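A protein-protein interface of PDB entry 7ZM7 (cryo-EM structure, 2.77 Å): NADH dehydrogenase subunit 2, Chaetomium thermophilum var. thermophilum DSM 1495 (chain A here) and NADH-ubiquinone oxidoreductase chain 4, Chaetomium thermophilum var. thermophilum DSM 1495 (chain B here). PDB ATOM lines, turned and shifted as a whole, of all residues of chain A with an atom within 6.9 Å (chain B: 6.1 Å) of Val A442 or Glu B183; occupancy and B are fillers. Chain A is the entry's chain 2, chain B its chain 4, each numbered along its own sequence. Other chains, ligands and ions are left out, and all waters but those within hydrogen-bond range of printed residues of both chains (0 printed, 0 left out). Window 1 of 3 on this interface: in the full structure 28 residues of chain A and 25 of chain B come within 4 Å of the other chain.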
ATOM      1  N   ILE A 436     -23.269   5.129 -29.728  1.00  0.00           N
ATOM      2  CA  ILE A 436     -23.931   3.837 -29.627  1.00  0.00           C
ATOM      3  C   ILE A 436     -23.196   2.923 -28.654  1.00  0.00           C
ATOM      4  O   ILE A 436     -23.813   2.185 -27.884  1.00  0.00           O
ATOM      5  CB  ILE A 436     -24.054   3.229 -31.036  1.00  0.00           C
ATOM      6  CG1 ILE A 436     -25.244   3.846 -31.754  1.00  0.00           C
ATOM      7  CG2 ILE A 436     -24.170   1.736 -30.992  1.00  0.00           C
ATOM      8  CD1 ILE A 436     -25.419   3.373 -33.116  1.00  0.00           C
ATOM      9  N   PHE A 437     -21.871   2.961 -28.663  1.00  0.00           N
ATOM     10  CA  PHE A 437     -21.120   2.207 -27.674  1.00  0.00           C
ATOM     11  C   PHE A 437     -21.376   2.707 -26.256  1.00  0.00           C
ATOM     12  O   PHE A 437     -21.170   1.960 -25.299  1.00  0.00           O
ATOM     13  CB  PHE A 437     -19.633   2.268 -27.997  1.00  0.00           C
ATOM     14  CG  PHE A 437     -19.222   1.362 -29.101  1.00  0.00           C
ATOM     15  CD1 PHE A 437     -19.396   0.000 -28.996  1.00  0.00           C
ATOM     16  CD2 PHE A 437     -18.661   1.871 -30.250  1.00  0.00           C
ATOM     17  CE1 PHE A 437     -19.029  -0.831 -30.017  1.00  0.00           C
ATOM     18  CE2 PHE A 437     -18.289   1.044 -31.272  1.00  0.00           C
ATOM     19  CZ  PHE A 437     -18.475  -0.314 -31.158  1.00  0.00           C
ATOM     20  N   SER A 438     -21.813   3.953 -26.100  1.00  0.00           N
ATOM     21  CA  SER A 438     -22.196   4.444 -24.785  1.00  0.00           C
ATOM     22  C   SER A 438     -23.529   3.840 -24.345  1.00  0.00           C
ATOM     23  O   SER A 438     -23.717   3.529 -23.168  1.00  0.00           O
ATOM     24  CB  SER A 438     -22.238   5.972 -24.809  1.00  0.00           C
ATOM     25  OG  SER A 438     -22.492   6.533 -23.542  1.00  0.00           O
ATOM     26  N   PHE A 439     -24.452   3.647 -25.286  1.00  0.00           N
ATOM     27  CA  PHE A 439     -25.689   2.929 -25.004  1.00  0.00           C
ATOM     28  C   PHE A 439     -25.421   1.489 -24.592  1.00  0.00           C
ATOM     29  O   PHE A 439     -26.118   0.948 -23.730  1.00  0.00           O
ATOM     30  CB  PHE A 439     -26.590   2.943 -26.237  1.00  0.00           C
ATOM     31  CG  PHE A 439     -27.106   4.292 -26.612  1.00  0.00           C
ATOM     32  CD1 PHE A 439     -27.203   5.302 -25.683  1.00  0.00           C
ATOM     33  CD2 PHE A 439     -27.520   4.539 -27.905  1.00  0.00           C
ATOM     34  CE1 PHE A 439     -27.690   6.521 -26.041  1.00  0.00           C
ATOM     35  CE2 PHE A 439     -28.002   5.753 -28.260  1.00  0.00           C
ATOM     36  CZ  PHE A 439     -28.093   6.743 -27.328  1.00  0.00           C
ATOM     37  N   VAL A 440     -24.446   0.835 -25.228  1.00  0.00           N
ATOM     38  CA  VAL A 440     -24.066  -0.524 -24.848  1.00  0.00           C
ATOM     39  C   VAL A 440     -23.517  -0.550 -23.432  1.00  0.00           C
ATOM     40  O   VAL A 440     -23.845  -1.439 -22.643  1.00  0.00           O
ATOM     41  CB  VAL A 440     -23.054  -1.102 -25.855  1.00  0.00           C
ATOM     42  CG1 VAL A 440     -22.611  -2.478 -25.423  1.00  0.00           C
ATOM     43  CG2 VAL A 440     -23.652  -1.168 -27.225  1.00  0.00           C
ATOM     44  N   GLY A 441     -22.708   0.443 -23.094  1.00  0.00           N
ATOM     45  CA  GLY A 441     -22.155   0.526 -21.736  1.00  0.00           C
ATOM     46  C   GLY A 441     -20.723   0.061 -21.746  1.00  0.00           C
ATOM     47  O   GLY A 441     -20.260  -0.400 -20.706  1.00  0.00           O
ATOM     48  N   VAL A 442     -19.988   0.319 -22.821  1.00  0.00           N
ATOM     49  CA  VAL A 442     -18.555  -0.080 -22.910  1.00  0.00           C
ATOM     50  C   VAL A 442     -17.671   1.025 -22.314  1.00  0.00           C
ATOM     51  O   VAL A 442     -17.884   2.184 -22.654  1.00  0.00           O
ATOM     52  CB  VAL A 442     -18.162  -0.442 -24.358  1.00  0.00           C
ATOM     53  CG1 VAL A 442     -17.139  -1.565 -24.398  1.00  0.00           C
ATOM     54  CG2 VAL A 442     -19.366  -0.800 -25.205  1.00  0.00           C
ATOM     55  N   PRO A 443     -16.702   0.710 -21.425  1.00  0.00           N
ATOM     56  CA  PRO A 443     -15.759   1.708 -20.886  1.00  0.00           C
ATOM     57  C   PRO A 443     -14.742   2.120 -21.967  1.00  0.00           C
ATOM     58  O   PRO A 443     -14.526   1.329 -22.847  1.00  0.00           O
ATOM     59  CB  PRO A 443     -15.040   0.951 -19.761  1.00  0.00           C
ATOM     60  CG  PRO A 443     -15.777  -0.355 -19.584  1.00  0.00           C
ATOM     61  CD  PRO A 443     -16.445  -0.631 -20.909  1.00  0.00           C
ATOM     62  N   PRO A 444     -14.171   3.346 -21.992  1.00  0.00           N
ATOM     63  CA  PRO A 444     -14.251   4.326 -20.897  1.00  0.00           C
ATOM     64  C   PRO A 444     -15.452   5.260 -21.064  1.00  0.00           C
ATOM     65  O   PRO A 444     -15.497   6.228 -20.361  1.00  0.00           O
ATOM     66  CB  PRO A 444     -12.963   5.123 -21.098  1.00  0.00           C
ATOM     67  CG  PRO A 444     -12.814   5.182 -22.597  1.00  0.00           C
ATOM     68  CD  PRO A 444     -13.363   3.862 -23.096  1.00  0.00           C
ATOM     69  N   LEU A 445     -16.375   4.930 -21.967  1.00  0.00           N
ATOM     70  CA  LEU A 445     -17.521   5.810 -22.309  1.00  0.00           C
ATOM     71  C   LEU A 445     -18.440   6.107 -21.128  1.00  0.00           C
ATOM     72  O   LEU A 445     -18.583   5.240 -20.264  1.00  0.00           O
ATOM     73  CB  LEU A 445     -18.250   5.226 -23.521  1.00  0.00           C
ATOM     74  CG  LEU A 445     -17.350   5.033 -24.741  1.00  0.00           C
ATOM     75  CD1 LEU A 445     -18.145   4.537 -25.928  1.00  0.00           C
ATOM     76  CD2 LEU A 445     -16.623   6.322 -25.093  1.00  0.00           C
ATOM     77  N   VAL A 446     -19.050   7.287 -21.123  1.00  0.00           N
ATOM     78  CA  VAL A 446     -19.914   7.772 -20.002  1.00  0.00           C
ATOM     79  C   VAL A 446     -21.036   6.788 -19.657  1.00  0.00           C
ATOM     80  O   VAL A 446     -21.364   6.695 -18.472  1.00  0.00           O
ATOM     81  CB  VAL A 446     -20.462   9.182 -20.317  1.00  0.00           C
ATOM     82  CG1 VAL A 446     -21.534   9.172 -21.392  1.00  0.00           C
ATOM     83  CG2 VAL A 446     -20.969   9.898 -19.075  1.00  0.00           C
ATOM     84  N   GLY A 447     -21.620   6.115 -20.648  1.00  0.00           N
ATOM     85  CA  GLY A 447     -22.746   5.254 -20.347  1.00  0.00           C
ATOM     86  C   GLY A 447     -22.354   4.017 -19.575  1.00  0.00           C
ATOM     87  O   GLY A 447     -23.212   3.349 -18.997  1.00  0.00           O
ATOM     88  N   PHE A 448     -21.063   3.678 -19.574  1.00  0.00           N
ATOM     89  CA  PHE A 448     -20.575   2.643 -18.676  1.00  0.00           C
ATOM     90  C   PHE A 448     -20.685   3.082 -17.231  1.00  0.00           C
ATOM     91  O   PHE A 448     -21.200   2.354 -16.379  1.00  0.00           O
ATOM     92  CB  PHE A 448     -19.128   2.303 -18.985  1.00  0.00           C
ATOM     93  CG  PHE A 448     -18.431   1.599 -17.856  1.00  0.00           C
ATOM     94  CD1 PHE A 448     -18.720   0.283 -17.572  1.00  0.00           C
ATOM     95  CD2 PHE A 448     -17.498   2.261 -17.077  1.00  0.00           C
ATOM     96  CE1 PHE A 448     -18.104  -0.354 -16.528  1.00  0.00           C
ATOM     97  CE2 PHE A 448     -16.864   1.625 -16.045  1.00  0.00           C
ATOM     98  CZ  PHE A 448     -17.174   0.316 -15.762  1.00  0.00           C
ATOM     99  N   PHE A 449     -20.184   4.269 -16.935  1.00  0.00           N
ATOM    100  CA  PHE A 449     -20.174   4.752 -15.573  1.00  0.00           C
ATOM    101  C   PHE A 449     -21.570   4.987 -15.039  1.00  0.00           C
ATOM    102  O   PHE A 449     -21.731   5.190 -13.841  1.00  0.00           O
ATOM    103  CB  PHE A 449     -19.351   6.023 -15.486  1.00  0.00           C
ATOM    104  CG  PHE A 449     -17.909   5.807 -15.721  1.00  0.00           C
ATOM    105  CD1 PHE A 449     -17.127   5.182 -14.767  1.00  0.00           C
ATOM    106  CD2 PHE A 449     -17.322   6.214 -16.897  1.00  0.00           C
ATOM    107  CE1 PHE A 449     -15.804   4.982 -14.976  1.00  0.00           C
ATOM    108  CE2 PHE A 449     -15.992   6.017 -17.103  1.00  0.00           C
ATOM    109  CZ  PHE A 449     -15.234   5.395 -16.138  1.00  0.00           C
ATOM    110  N   LYS A 451     -24.295   2.691 -15.881  1.00  0.00           N
ATOM    111  CA  LYS A 451     -24.750   1.345 -15.550  1.00  0.00           C
ATOM    112  C   LYS A 451     -23.944   0.750 -14.412  1.00  0.00           C
ATOM    113  O   LYS A 451     -24.482  -0.015 -13.611  1.00  0.00           O
ATOM    114  CB  LYS A 451     -24.664   0.436 -16.776  1.00  0.00           C
ATOM    115  CG  LYS A 451     -25.634   0.770 -17.889  1.00  0.00           C
ATOM    116  CD  LYS A 451     -25.309  -0.054 -19.115  1.00  0.00           C
ATOM    117  CE  LYS A 451     -26.300   0.150 -20.246  1.00  0.00           C
ATOM    118  NZ  LYS A 451     -25.951  -0.639 -21.446  1.00  0.00           N
ATOM    119  N   PHE B 178      -8.539  -1.283 -13.840  1.00  0.00           N
ATOM    120  CA  PHE B 178      -8.138  -2.437 -14.633  1.00  0.00           C
ATOM    121  C   PHE B 178      -9.258  -2.883 -15.550  1.00  0.00           C
ATOM    122  O   PHE B 178      -9.032  -3.124 -16.738  1.00  0.00           O
ATOM    123  CB  PHE B 178      -7.707  -3.573 -13.708  1.00  0.00           C
ATOM    124  CG  PHE B 178      -7.437  -4.872 -14.404  1.00  0.00           C
ATOM    125  CD1 PHE B 178      -6.219  -5.122 -14.974  1.00  0.00           C
ATOM    126  CD2 PHE B 178      -8.390  -5.861 -14.449  1.00  0.00           C
ATOM    127  CE1 PHE B 178      -5.973  -6.326 -15.596  1.00  0.00           C
ATOM    128  CE2 PHE B 178      -8.139  -7.055 -15.074  1.00  0.00           C
ATOM    129  CZ  PHE B 178      -6.934  -7.286 -15.634  1.00  0.00           C
ATOM    130  N   TYR B 179     -10.479  -2.974 -15.018  1.00  0.00           N
ATOM    131  CA  TYR B 179     -11.636  -3.382 -15.803  1.00  0.00           C
ATOM    132  C   TYR B 179     -11.951  -2.388 -16.906  1.00  0.00           C
ATOM    133  O   TYR B 179     -12.413  -2.782 -17.977  1.00  0.00           O
ATOM    134  CB  TYR B 179     -12.852  -3.554 -14.885  1.00  0.00           C
ATOM    135  CG  TYR B 179     -14.131  -3.868 -15.613  1.00  0.00           C
ATOM    136  CD1 TYR B 179     -14.960  -2.857 -16.077  1.00  0.00           C
ATOM    137  CD2 TYR B 179     -14.503  -5.164 -15.848  1.00  0.00           C
ATOM    138  CE1 TYR B 179     -16.096  -3.134 -16.751  1.00  0.00           C
ATOM    139  CE2 TYR B 179     -15.645  -5.449 -16.514  1.00  0.00           C
ATOM    140  CZ  TYR B 179     -16.439  -4.434 -16.965  1.00  0.00           C
ATOM    141  OH  TYR B 179     -17.591  -4.727 -17.639  1.00  0.00           O
ATOM    142  N   ILE B 180     -11.724  -1.101 -16.661  1.00  0.00           N
ATOM    143  CA  ILE B 180     -12.065  -0.076 -17.640  1.00  0.00           C
ATOM    144  C   ILE B 180     -11.245  -0.254 -18.904  1.00  0.00           C
ATOM    145  O   ILE B 180     -11.779  -0.234 -20.016  1.00  0.00           O
ATOM    146  CB  ILE B 180     -11.877   1.324 -17.037  1.00  0.00           C
ATOM    147  CG1 ILE B 180     -12.992   1.613 -16.041  1.00  0.00           C
ATOM    148  CG2 ILE B 180     -11.847   2.366 -18.120  1.00  0.00           C
ATOM    149  CD1 ILE B 180     -12.726   2.753 -15.147  1.00  0.00           C
ATOM    150  N   PHE B 181      -9.935  -0.430 -18.753  1.00  0.00           N
ATOM    151  CA  PHE B 181      -9.076  -0.640 -19.906  1.00  0.00           C
ATOM    152  C   PHE B 181      -9.145  -2.063 -20.427  1.00  0.00           C
ATOM    153  O   PHE B 181      -8.971  -2.287 -21.625  1.00  0.00           O
ATOM    154  CB  PHE B 181      -7.652  -0.266 -19.547  1.00  0.00           C
ATOM    155  CG  PHE B 181      -7.517   1.155 -19.164  1.00  0.00           C
ATOM    156  CD1 PHE B 181      -7.932   2.137 -20.026  1.00  0.00           C
ATOM    157  CD2 PHE B 181      -7.029   1.515 -17.938  1.00  0.00           C
ATOM    158  CE1 PHE B 181      -7.849   3.434 -19.687  1.00  0.00           C
ATOM    159  CE2 PHE B 181      -6.943   2.813 -17.611  1.00  0.00           C
ATOM    160  CZ  PHE B 181      -7.354   3.776 -18.488  1.00  0.00           C
ATOM    161  N   PHE B 182      -9.390  -3.036 -19.548  1.00  0.00           N
ATOM    162  CA  PHE B 182      -9.522  -4.458 -19.965  1.00  0.00           C
ATOM    163  C   PHE B 182     -10.705  -4.586 -20.925  1.00  0.00           C
ATOM    164  O   PHE B 182     -10.776  -5.596 -21.639  1.00  0.00           O
ATOM    165  CB  PHE B 182      -9.654  -5.344 -18.722  1.00  0.00           C
ATOM    166  CG  PHE B 182      -9.980  -6.803 -18.909  1.00  0.00           C
ATOM    167  CD1 PHE B 182     -11.278  -7.264 -18.764  1.00  0.00           C
ATOM    168  CD2 PHE B 182      -8.981  -7.729 -19.155  1.00  0.00           C
ATOM    169  CE1 PHE B 182     -11.576  -8.610 -18.912  1.00  0.00           C
ATOM    170  CE2 PHE B 182      -9.279  -9.076 -19.299  1.00  0.00           C
ATOM    171  CZ  PHE B 182     -10.576  -9.514 -19.179  1.00  0.00           C
ATOM    172  N   GLU B 183     -11.568  -3.569 -20.989  1.00  0.00           N
ATOM    173  CA  GLU B 183     -12.791  -3.676 -21.829  1.00  0.00           C
ATOM    174  C   GLU B 183     -12.914  -2.485 -22.778  1.00  0.00           C
ATOM    175  O   GLU B 183     -13.913  -2.451 -23.515  1.00  0.00           O
ATOM    176  CB  GLU B 183     -14.031  -3.846 -20.953  1.00  0.00           C
ATOM    177  CG  GLU B 183     -14.167  -5.254 -20.416  1.00  0.00           C
ATOM    178  CD  GLU B 183     -14.037  -6.326 -21.487  1.00  0.00           C
ATOM    179  OE1 GLU B 183     -14.797  -6.271 -22.467  1.00  0.00           O
ATOM    180  OE2 GLU B 183     -13.179  -7.215 -21.340  1.00  0.00           O
ATOM    181  N   SER B 184     -11.969  -1.544 -22.778  1.00  0.00           N
ATOM    182  CA  SER B 184     -11.965  -0.474 -23.763  1.00  0.00           C
ATOM    183  C   SER B 184     -11.410  -0.961 -25.090  1.00  0.00           C
ATOM    184  O   SER B 184     -11.698  -0.373 -26.132  1.00  0.00           O
ATOM    185  CB  SER B 184     -11.177   0.730 -23.248  1.00  0.00           C
ATOM    186  OG  SER B 184      -9.867   0.373 -22.871  1.00  0.00           O
ATOM    187  N   ILE B 185     -10.740  -2.105 -25.065  1.00  0.00           N
ATOM    188  CA  ILE B 185     -10.071  -2.687 -26.259  1.00  0.00           C
ATOM    189  C   ILE B 185     -11.156  -3.314 -27.125  1.00  0.00           C
ATOM    190  O   ILE B 185     -10.849  -3.679 -28.263  1.00  0.00           O
ATOM    191  CB  ILE B 185      -9.032  -3.734 -25.817  1.00  0.00           C
ATOM    192  CG1 ILE B 185      -9.702  -4.930 -25.136  1.00  0.00           C
ATOM    193  CG2 ILE B 185      -7.971  -3.106 -24.928  1.00  0.00           C
ATOM    194  CD1 ILE B 185      -8.797  -6.120 -24.966  1.00  0.00           C
ATOM    195  N   LEU B 186     -12.397  -3.353 -26.639  1.00  0.00           N
ATOM    196  CA  LEU B 186     -13.439  -4.113 -27.321  1.00  0.00           C
ATOM    197  C   LEU B 186     -13.988  -3.396 -28.553  1.00  0.00           C
ATOM    198  O   LEU B 186     -14.173  -4.057 -29.585  1.00  0.00           O
ATOM    199  CB  LEU B 186     -14.525  -4.477 -26.301  1.00  0.00           C
ATOM    200  CG  LEU B 186     -15.461  -5.669 -26.471  1.00  0.00           C
ATOM    201  CD1 LEU B 186     -14.690  -6.919 -26.784  1.00  0.00           C
ATOM    202  CD2 LEU B 186     -16.251  -5.844 -25.192  1.00  0.00           C
ATOM    203  N   PRO B 187     -14.287  -2.096 -28.528  1.00  0.00           N
ATOM    204  CA  PRO B 187     -14.785  -1.428 -29.742  1.00  0.00           C
ATOM    205  C   PRO B 187     -13.767  -1.386 -30.872  1.00  0.00           C
ATOM    206  O   PRO B 187     -14.122  -1.705 -32.016  1.00  0.00           O
ATOM    207  CB  PRO B 187     -15.140  -0.022 -29.246  1.00  0.00           C
ATOM    208  CG  PRO B 187     -15.529  -0.246 -27.898  1.00  0.00           C
ATOM    209  CD  PRO B 187     -14.582  -1.266 -27.354  1.00  0.00           C
ATOM    210  N   PHE B 209     -16.727  -9.792 -29.600  1.00  0.00           N
ATOM    211  CA  PHE B 209     -17.293  -8.660 -28.835  1.00  0.00           C
ATOM    212  C   PHE B 209     -18.296  -9.212 -27.829  1.00  0.00           C
ATOM    213  O   PHE B 209     -18.110  -8.962 -26.637  1.00  0.00           O
ATOM    214  CB  PHE B 209     -17.976  -7.632 -29.744  1.00  0.00           C
ATOM    215  CG  PHE B 209     -18.345  -6.336 -29.064  1.00  0.00           C
ATOM    216  CD1 PHE B 209     -19.442  -6.257 -28.220  1.00  0.00           C
ATOM    217  CD2 PHE B 209     -17.594  -5.191 -29.271  1.00  0.00           C
ATOM    218  CE1 PHE B 209     -19.774  -5.067 -27.593  1.00  0.00           C
ATOM    219  CE2 PHE B 209     -17.927  -4.001 -28.644  1.00  0.00           C
ATOM    220  CZ  PHE B 209     -19.016  -3.941 -27.806  1.00  0.00           C
ATOM    221  N   THR B 212     -16.867 -11.539 -25.055  1.00  0.00           N
ATOM    222  CA  THR B 212     -15.945 -10.780 -24.176  1.00  0.00           C
ATOM    223  C   THR B 212     -16.773  -9.746 -23.426  1.00  0.00           C
ATOM    224  O   THR B 212     -16.368  -9.372 -22.320  1.00  0.00           O
ATOM    225  CB  THR B 212     -14.781 -10.193 -24.986  1.00  0.00           C
ATOM    226  OG1 THR B 212     -14.211 -11.261 -25.740  1.00  0.00           O
ATOM    227  CG2 THR B 212     -13.697  -9.561 -24.146  1.00  0.00           C
ATOM    228  N   LEU B 213     -17.897  -9.314 -24.002  1.00  0.00           N
ATOM    229  CA  LEU B 213     -18.717  -8.400 -23.219  1.00  0.00           C
ATOM    230  C   LEU B 213     -19.438  -9.135 -22.111  1.00  0.00           C
ATOM    231  O   LEU B 213     -19.517  -8.644 -20.984  1.00  0.00           O
ATOM    232  CB  LEU B 213     -19.737  -7.687 -24.108  1.00  0.00           C
ATOM    233  CG  LEU B 213     -20.643  -6.709 -23.357  1.00  0.00           C
ATOM    234  CD1 LEU B 213     -19.870  -5.550 -22.811  1.00  0.00           C
ATOM    235  CD2 LEU B 213     -21.781  -6.263 -24.203  1.00  0.00           C
ATOM    236  N   SER B 216     -17.050 -10.369 -19.282  1.00  0.00           N
ATOM    237  CA  SER B 216     -16.519  -9.254 -18.515  1.00  0.00           C
ATOM    238  C   SER B 216     -17.554  -8.625 -17.598  1.00  0.00           C
ATOM    239  O   SER B 216     -17.180  -7.908 -16.676  1.00  0.00           O
ATOM    240  CB  SER B 216     -15.948  -8.201 -19.454  1.00  0.00           C
ATOM    241  OG  SER B 216     -16.957  -7.397 -20.025  1.00  0.00           O
ATOM    242  N   LYS B 262     -12.230 -15.725 -20.955  1.00  0.00           N
ATOM    243  CA  LYS B 262     -11.118 -14.971 -21.600  1.00  0.00           C
ATOM    244  C   LYS B 262      -9.799 -15.752 -21.630  1.00  0.00           C
ATOM    245  O   LYS B 262      -8.820 -15.193 -22.148  1.00  0.00           O
ATOM    246  CB  LYS B 262     -10.976 -13.575 -20.990  1.00  0.00           C
ATOM    247  CG  LYS B 262     -11.848 -12.505 -21.628  1.00  0.00           C
ATOM    248  CD  LYS B 262     -11.817 -12.533 -23.146  1.00  0.00           C
ATOM    249  CE  LYS B 262     -10.597 -11.873 -23.756  1.00  0.00           C
ATOM    250  NZ  LYS B 262      -9.530 -12.849 -24.076  1.00  0.00           N
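Printed residues of chain A that touch a printed residue of chain B: Phe A437, Val A442, Pro A443, Pro A444, Phe A448 and Phe A449. Hydrophobic or aromatic side chains of chain A within 4 Å of the printed part of chain B: Phe A437, Val A442, Pro A443, Pro A444, Phe A448 and Phe A449. Hydrophobic or aromatic side chains of chain B within 4 Å of the printed part of chain A: Tyr B179, Ile B180, Pro B187 and Phe B209. Among the printed residues, 12 pairs touch across the chains. Among the printed residues, no Asp or Glu carboxylate lies within 4 Å of a Lys or Arg side-chain nitrogen of the other chain.
Phe A437 touches Pro B187 (CZ to CB, 3.9 Å). Phe A437 touches Phe B209 (CE1 to CE2, 3.6 Å). Val A442 touches Glu B183. CG1 of Val A442 touches CD of Pro B187, 3.9 Å away. CE1 of Tyr B179 touches CG of Pro A443 (3.98 Å). CB of Pro A443 touches O of Ile B180, at 3.5 Å. Pro A443 touches Glu B183 (O to O, 3.9 Å). Ser B184 touches Pro A444 (CB to CD, 3.8 Å). CE1 of Tyr B179 touches CE1 of Phe A448, 3.4 Å away. Phe A448 touches Ile B180.
Of the printed residues of chain B, Pro A444 touches Ser B184. Printed residues of chain B within 4 Å of Phe A448: Tyr B179 and Ile B180. Of the printed residues of chain B, Phe A449 touches Ile B180. Of the printed residues of chain A, Tyr B179 touches Pro A443 and Phe A448. Glu B183 touches two residues of chain A. The nearest residue of chain B that does not touch Val A442 is Phe B209 (4.1 Å). The nearest printed residue of chain B that does not touch Phe A437 is Leu B186 (5.8 Å).
The backbone carbonyl oxygen of Phe A437 is in hydrogen-bond range of the backbone NH of Val A442 (3.2 Å). The side-chain hydroxyl (OH) of Tyr B179 lies close to the backbone carbonyl oxygen (O) of Ser B216. O of Ile B180 sits close to OG of Ser B184, 3.5 Å away. The backbone carbonyl oxygen of Phe B181 is in hydrogen-bond range of the side-chain hydroxyl of Ser B184 (3.1 Å). The side-chain carboxylate (OE1) of Glu B183 sits close to the side-chain hydroxyl (OG) of Ser B216, 3.4 Å away.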
